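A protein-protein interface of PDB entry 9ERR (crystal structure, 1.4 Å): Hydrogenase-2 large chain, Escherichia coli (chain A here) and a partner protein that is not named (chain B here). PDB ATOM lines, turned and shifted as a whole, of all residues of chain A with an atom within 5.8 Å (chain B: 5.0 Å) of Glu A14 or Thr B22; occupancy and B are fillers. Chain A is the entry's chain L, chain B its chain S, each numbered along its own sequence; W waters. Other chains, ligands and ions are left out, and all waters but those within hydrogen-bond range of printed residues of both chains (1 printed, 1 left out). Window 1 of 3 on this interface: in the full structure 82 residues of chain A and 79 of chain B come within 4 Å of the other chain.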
ATOM      1  N   ARG A  12       4.726   8.990  26.972  1.00  0.00           N
ATOM      2  CA  ARG A  12       3.737   7.930  26.921  1.00  0.00           C
ATOM      3  C   ARG A  12       3.096   7.798  28.296  1.00  0.00           C
ATOM      4  O   ARG A  12       2.808   6.682  28.762  1.00  0.00           O
ATOM      5  CB  ARG A  12       4.303   6.649  26.322  1.00  0.00           C
ATOM      6  CG  ARG A  12       4.350   6.716  24.801  1.00  0.00           C
ATOM      7  CD  ARG A  12       4.879   5.458  24.187  1.00  0.00           C
ATOM      8  NE  ARG A  12       6.273   5.238  24.529  1.00  0.00           N
ATOM      9  CZ  ARG A  12       6.758   4.187  25.198  1.00  0.00           C
ATOM     10  NH1 ARG A  12       5.948   3.278  25.701  1.00  0.00           N
ATOM     11  NH2 ARG A  12       8.070   4.069  25.391  1.00  0.00           N
ATOM     12  N   ILE A  13       2.845   8.968  28.879  1.00  0.00           N
ATOM     13  CA  ILE A  13       1.980   9.115  30.034  1.00  0.00           C
ATOM     14  C   ILE A  13       1.085  10.309  29.726  1.00  0.00           C
ATOM     15  O   ILE A  13       1.192  10.963  28.681  1.00  0.00           O
ATOM     16  CB  ILE A  13       2.780   9.359  31.331  1.00  0.00           C
ATOM     17  CG1 ILE A  13       3.594  10.650  31.216  1.00  0.00           C
ATOM     18  CG2 ILE A  13       3.666   8.178  31.692  1.00  0.00           C
ATOM     19  CD1 ILE A  13       4.051  11.154  32.495  1.00  0.00           C
ATOM     20  N   GLU A  14       0.159  10.606  30.622  1.00  0.00           N
ATOM     21  CA  GLU A  14      -0.470  11.912  30.585  1.00  0.00           C
ATOM     22  C   GLU A  14       0.337  12.847  31.463  1.00  0.00           C
ATOM     23  O   GLU A  14       0.576  12.567  32.649  1.00  0.00           O
ATOM     24  CB  GLU A  14      -1.909  11.834  31.101  1.00  0.00           C
ATOM     25  CG  GLU A  14      -2.685  13.136  30.941  1.00  0.00           C
ATOM     26  CD  GLU A  14      -2.193  14.333  31.728  1.00  0.00           C
ATOM     27  OE1 GLU A  14      -1.761  14.124  32.873  1.00  0.00           O
ATOM     28  OE2 GLU A  14      -2.243  15.528  31.212  1.00  0.00           O
ATOM     29  N   GLY A  15       0.667  13.987  30.904  1.00  0.00           N
ATOM     30  CA  GLY A  15       1.231  15.068  31.679  1.00  0.00           C
ATOM     31  C   GLY A  15       2.750  14.998  31.820  1.00  0.00           C
ATOM     32  O   GLY A  15       3.477  14.282  31.088  1.00  0.00           O
ATOM     33  N   HIS A  16       3.188  15.787  32.765  1.00  0.00           N
ATOM     34  CA  HIS A  16       4.569  16.132  32.948  1.00  0.00           C
ATOM     35  C   HIS A  16       5.151  15.446  34.181  1.00  0.00           C
ATOM     36  O   HIS A  16       4.814  15.811  35.297  1.00  0.00           O
ATOM     37  CB  HIS A  16       4.657  17.664  33.035  1.00  0.00           C
ATOM     38  CG  HIS A  16       4.199  18.409  31.815  1.00  0.00           C
ATOM     39  ND1 HIS A  16       4.813  18.338  30.592  1.00  0.00           N
ATOM     40  CD2 HIS A  16       3.141  19.213  31.617  1.00  0.00           C
ATOM     41  CE1 HIS A  16       4.184  19.116  29.731  1.00  0.00           C
ATOM     42  NE2 HIS A  16       3.164  19.667  30.326  1.00  0.00           N
ATOM     43  N   ILE A  60      -9.435  18.912  35.089  1.00  0.00           N
ATOM     44  CA  ILE A  60      -8.225  18.356  35.668  1.00  0.00           C
ATOM     45  C   ILE A  60      -7.541  17.400  34.680  1.00  0.00           C
ATOM     46  O   ILE A  60      -6.292  17.391  34.578  1.00  0.00           O
ATOM     47  CB  ILE A  60      -8.527  17.647  37.010  1.00  0.00           C
ATOM     48  CG1 ILE A  60      -8.803  18.680  38.108  1.00  0.00           C
ATOM     49  CG2 ILE A  60      -7.439  16.693  37.403  1.00  0.00           C
ATOM     50  CD1 ILE A  60      -9.320  18.130  39.400  1.00  0.00           C
ATOM     51  N   CYS A  61      -8.337  16.647  33.902  1.00  0.00           N
ATOM     52  CA  CYS A  61      -7.718  15.714  32.968  1.00  0.00           C
ATOM     53  C   CYS A  61      -8.662  15.339  31.827  1.00  0.00           C
ATOM     54  O   CYS A  61      -9.838  15.024  32.055  1.00  0.00           O
ATOM     55  CB  CYS A  61      -7.283  14.489  33.746  1.00  0.00           C
ATOM     56  SG  CYS A  61      -6.349  13.277  32.783  1.00  0.00           S
ATOM     57  N   GLY A  62      -8.060  15.262  30.630  1.00  0.00           N
ATOM     58  CA  GLY A  62      -8.773  14.867  29.439  1.00  0.00           C
ATOM     59  C   GLY A  62      -8.486  13.452  29.007  1.00  0.00           C
ATOM     60  O   GLY A  62      -9.159  12.989  28.078  1.00  0.00           O
ATOM     61  N   VAL A  63      -7.472  12.814  29.595  1.00  0.00           N
ATOM     62  CA  VAL A  63      -7.289  11.396  29.336  1.00  0.00           C
ATOM     63  C   VAL A  63      -8.347  10.643  30.136  1.00  0.00           C
ATOM     64  O   VAL A  63      -9.189   9.972  29.552  1.00  0.00           O
ATOM     65  CB  VAL A  63      -5.884  10.912  29.673  1.00  0.00           C
ATOM     66  CG1 VAL A  63      -5.775   9.410  29.515  1.00  0.00           C
ATOM     67  CG2 VAL A  63      -4.835  11.611  28.823  1.00  0.00           C
ATOM     68  N   LEU A 111       0.190   3.701  24.874  1.00  0.00           N
ATOM     69  CA  LEU A 111       1.085   4.235  25.895  1.00  0.00           C
ATOM     70  C   LEU A 111       2.161   3.213  26.278  1.00  0.00           C
ATOM     71  O   LEU A 111       3.310   3.605  26.486  1.00  0.00           O
ATOM     72  CB  LEU A 111       0.305   4.758  27.099  1.00  0.00           C
ATOM     73  CG  LEU A 111      -0.751   5.818  26.772  1.00  0.00           C
ATOM     74  CD1 LEU A 111      -1.467   6.245  28.043  1.00  0.00           C
ATOM     75  CD2 LEU A 111      -0.151   7.021  26.050  1.00  0.00           C
ATOM     76  N   PRO A 545       0.578   6.458  34.732  1.00  0.00           N
ATOM     77  CA  PRO A 545       0.647   7.782  35.321  1.00  0.00           C
ATOM     78  C   PRO A 545      -0.203   8.805  34.576  1.00  0.00           C
ATOM     79  O   PRO A 545      -0.189   8.942  33.349  1.00  0.00           O
ATOM     80  CB  PRO A 545       2.114   8.172  35.316  1.00  0.00           C
ATOM     81  CG  PRO A 545       2.824   6.848  35.161  1.00  0.00           C
ATOM     82  CD  PRO A 545       1.909   5.969  34.333  1.00  0.00           C
ATOM     83  N   CYS A 546      -0.864   9.626  35.390  1.00  0.00           N
ATOM     84  CA  CYS A 546      -1.530  10.818  34.895  1.00  0.00           C
ATOM     85  C   CYS A 546      -1.176  11.982  35.821  1.00  0.00           C
ATOM     86  O   CYS A 546      -1.644  12.038  36.961  1.00  0.00           O
ATOM     87  CB  CYS A 546      -3.024  10.608  34.855  1.00  0.00           C
ATOM     88  SG  CYS A 546      -3.861  12.051  34.160  1.00  0.00           S
ATOM     89  N   MET A 547      -0.330  12.920  35.343  1.00  0.00           N
ATOM     90  CA  MET A 547       0.234  13.927  36.247  1.00  0.00           C
ATOM     91  C   MET A 547      -0.614  15.204  36.292  1.00  0.00           C
ATOM     92  O   MET A 547      -0.562  15.940  37.292  1.00  0.00           O
ATOM     93  CB  MET A 547       1.686  14.283  35.889  1.00  0.00           C
ATOM     94  CG  MET A 547       2.586  13.070  35.862  1.00  0.00           C
ATOM     95  SD  MET A 547       2.461  11.972  37.288  1.00  0.00           S
ATOM     96  CE  MET A 547       3.097  13.050  38.563  1.00  0.00           C
ATOM     97  N   ALA A 548      -1.477  15.412  35.290  1.00  0.00           N
ATOM     98  CA  ALA A 548      -2.508  16.446  35.388  1.00  0.00           C
ATOM     99  C   ALA A 548      -3.442  16.040  36.528  1.00  0.00           C
ATOM    100  O   ALA A 548      -3.832  16.832  37.404  1.00  0.00           O
ATOM    101  CB  ALA A 548      -3.247  16.595  34.060  1.00  0.00           C
ATOM    102  N   CYS A 549      -3.806  14.757  36.548  1.00  0.00           N
ATOM    103  CA  CYS A 549      -4.548  14.189  37.660  1.00  0.00           C
ATOM    104  C   CYS A 549      -3.793  14.283  38.978  1.00  0.00           C
ATOM    105  O   CYS A 549      -4.348  14.687  39.986  1.00  0.00           O
ATOM    106  CB  CYS A 549      -4.860  12.726  37.399  1.00  0.00           C
ATOM    107  SG  CYS A 549      -6.378  12.506  36.425  1.00  0.00           S
ATOM    108  N   GLU B  20      -1.511  21.597  30.051  1.00  0.00           N
ATOM    109  CA  GLU B  20      -2.541  20.924  29.268  1.00  0.00           C
ATOM    110  C   GLU B  20      -3.114  19.732  30.033  1.00  0.00           C
ATOM    111  O   GLU B  20      -2.366  19.034  30.720  1.00  0.00           O
ATOM    112  CB  GLU B  20      -1.955  20.430  27.946  1.00  0.00           C
ATOM    113  CG  GLU B  20      -1.345  19.036  28.005  1.00  0.00           C
ATOM    114  CD  GLU B  20       0.092  18.942  28.477  1.00  0.00           C
ATOM    115  OE1 GLU B  20       0.580  19.920  29.052  1.00  0.00           O
ATOM    116  OE2 GLU B  20       0.727  17.888  28.243  1.00  0.00           O
ATOM    117  N   CYS B  21      -4.429  19.479  29.860  1.00  0.00           N
ATOM    118  CA  CYS B  21      -5.084  18.358  30.513  1.00  0.00           C
ATOM    119  C   CYS B  21      -4.995  17.106  29.633  1.00  0.00           C
ATOM    120  O   CYS B  21      -5.435  16.045  30.050  1.00  0.00           O
ATOM    121  CB  CYS B  21      -6.539  18.686  30.861  1.00  0.00           C
ATOM    122  SG  CYS B  21      -7.656  18.511  29.452  1.00  0.00           S
ATOM    123  N   THR B  22      -4.494  17.257  28.395  1.00  0.00           N
ATOM    124  CA  THR B  22      -4.328  16.212  27.379  1.00  0.00           C
ATOM    125  C   THR B  22      -5.618  15.993  26.567  1.00  0.00           C
ATOM    126  O   THR B  22      -5.607  15.253  25.584  1.00  0.00           O
ATOM    127  CB  THR B  22      -3.687  14.915  27.890  1.00  0.00           C
ATOM    128  OG1 THR B  22      -2.586  15.350  28.691  1.00  0.00           O
ATOM    129  CG2 THR B  22      -3.154  13.983  26.827  1.00  0.00           C
ATOM    130  N   GLY B  23      -6.705  16.669  26.911  1.00  0.00           N
ATOM    131  CA  GLY B  23      -7.955  16.523  26.182  1.00  0.00           C
ATOM    132  C   GLY B  23      -7.831  16.920  24.710  1.00  0.00           C
ATOM    133  O   GLY B  23      -8.527  16.386  23.844  1.00  0.00           O
ATOM    134  N   CYS B  24      -6.980  17.903  24.419  1.00  0.00           N
ATOM    135  CA  CYS B  24      -6.800  18.378  23.055  1.00  0.00           C
ATOM    136  C   CYS B  24      -6.072  17.323  22.217  1.00  0.00           C
ATOM    137  O   CYS B  24      -6.456  17.071  21.086  1.00  0.00           O
ATOM    138  CB  CYS B  24      -6.087  19.735  23.018  1.00  0.00           C
ATOM    139  SG  CYS B  24      -7.100  21.116  23.588  1.00  0.00           S
ATOM    140  N   THR B  25      -5.056  16.644  22.773  1.00  0.00           N
ATOM    141  CA  THR B  25      -4.471  15.500  22.085  1.00  0.00           C
ATOM    142  C   THR B  25      -5.522  14.399  21.922  1.00  0.00           C
ATOM    143  O   THR B  25      -5.638  13.738  20.872  1.00  0.00           O
ATOM    144  CB  THR B  25      -3.237  14.971  22.837  1.00  0.00           C
ATOM    145  OG1 THR B  25      -2.194  15.944  22.653  1.00  0.00           O
ATOM    146  CG2 THR B  25      -2.822  13.590  22.383  1.00  0.00           C
ATOM    147  N   GLU B  26      -6.227  14.115  23.012  1.00  0.00           N
ATOM    148  CA  GLU B  26      -7.250  13.064  22.989  1.00  0.00           C
ATOM    149  C   GLU B  26      -8.316  13.285  21.924  1.00  0.00           C
ATOM    150  O   GLU B  26      -8.877  12.309  21.437  1.00  0.00           O
ATOM    151  CB  GLU B  26      -7.872  12.944  24.380  1.00  0.00           C
ATOM    152  CG  GLU B  26      -7.018  12.181  25.351  1.00  0.00           C
ATOM    153  CD  GLU B  26      -6.981  10.683  25.219  1.00  0.00           C
ATOM    154  OE1 GLU B  26      -7.620  10.115  24.349  1.00  0.00           O
ATOM    155  OE2 GLU B  26      -6.210  10.078  26.014  1.00  0.00           O
ATOM    156  N   VAL B  51       2.998  12.385  24.315  1.00  0.00           N
ATOM    157  CA  VAL B  51       2.025  11.367  24.687  1.00  0.00           C
ATOM    158  C   VAL B  51       2.259  10.063  23.910  1.00  0.00           C
ATOM    159  O   VAL B  51       1.985   8.985  24.430  1.00  0.00           O
ATOM    160  CB  VAL B  51       0.588  11.891  24.516  1.00  0.00           C
ATOM    161  CG1 VAL B  51      -0.464  10.837  24.823  1.00  0.00           C
ATOM    162  CG2 VAL B  51       0.322  13.119  25.379  1.00  0.00           C
ATOM    163  N   ASP B  80      -0.907  22.944  23.118  1.00  0.00           N
ATOM    164  CA  ASP B  80      -2.066  22.882  23.987  1.00  0.00           C
ATOM    165  C   ASP B  80      -1.685  23.256  25.416  1.00  0.00           C
ATOM    166  O   ASP B  80      -0.529  23.089  25.844  1.00  0.00           O
ATOM    167  CB  ASP B  80      -2.789  21.532  23.914  1.00  0.00           C
ATOM    168  CG  ASP B  80      -1.978  20.282  24.205  1.00  0.00           C
ATOM    169  OD1 ASP B  80      -0.741  20.348  24.198  1.00  0.00           O
ATOM    170  OD2 ASP B  80      -2.611  19.220  24.363  1.00  0.00           O
HETATM  171  O   HOH W   1       0.287  15.067  28.336  1.00  0.00           O
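Water W1 lies within hydrogen-bond range of the backbone NH (N) of Gly A15 (2.8 Å), the side-chain carboxylate (OE2) of Glu B20 (2.9 Å) and the side-chain hydroxyl (OG1) of Thr B22 (2.9 Å).
The backbone NH (N) of Gly A62 is in hydrogen-bond range of the backbone carbonyl oxygen (O) of Cys B21, 2.8 Å away.
A ring nitrogen (NE2) of His A16 sits at hydrogen-bond distance from the side-chain carboxylate of Glu B20, 2.9 Å away.
OG1 of Thr B22 lies within hydrogen-bond range of OE2 of Glu A14 (2.6 Å).
O of Cys B21 sits close to OE2 of Glu A14.
Among the printed residues, pairs that only touch across the chains: Arg A12 with Val B51 (3.2 Å), Leu A111 with Val B51 (3.3 Å), Val A63 with Glu B26 (3.5 Å), Val A63 with Thr B22 (3.5 Å), Glu A14 with Glu B20 (3.5 Å), Gly A62 with Glu B26 (3.6 Å), Cys A61 with Cys B21 (3.7 Å), Gly A62 with Gly B23 (3.7 Å), Val A63 with Cys B21 (3.8 Å) and Ile A60 with Cys B21 (3.9 Å).
Of the 15 printed residues of chain A, 8 touch a printed residue of chain B.
Hydrophobic or aromatic side chains of chain A that line the printed part of chain B: His A16, Val A63 and Leu A111.
Printed residues of chain B within 4 Å of Glu A14: Glu B20, Cys B21 and Thr B22.
Thr B22 touches just these residues of chain A: Glu A14 and Val A63.
Of the printed residues of chain B, Leu A111 touches Val B51 (3.3 Å).
Of the printed residues of chain A, Glu B20 touches Glu A14 (3.5 Å) and His A16 (2.9 Å).
Of the printed residues of chain A, Glu B26 touches Gly A62 and Val A63.
Ile A13 touches none of the printed residues of chain B.
The nearest residue of chain A that does not touch Thr B22 is Gly A15 (4.2 Å).
The nearest printed residue of chain A that does not touch Val B51 is Ile A13 (4.04 Å).
N of Gly B23 lies close to SG of Cys B21 (3.3 Å).
The guanidinium group (NH1) of Arg A12 lies within hydrogen-bond range of the backbone carbonyl oxygen (O) of Leu A111 (2.8 Å).
O of Glu A14 lies within hydrogen-bond range of N of Met A547.
SG of Cys A61 lies close to N of Val A63.
OE1 of Glu A14 lies close to SG of Cys A546, 3.2 Å away.
The side-chain carboxylate (OE1) of Glu A14 lies within hydrogen-bond range of the backbone NH (N) of Ala A548.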
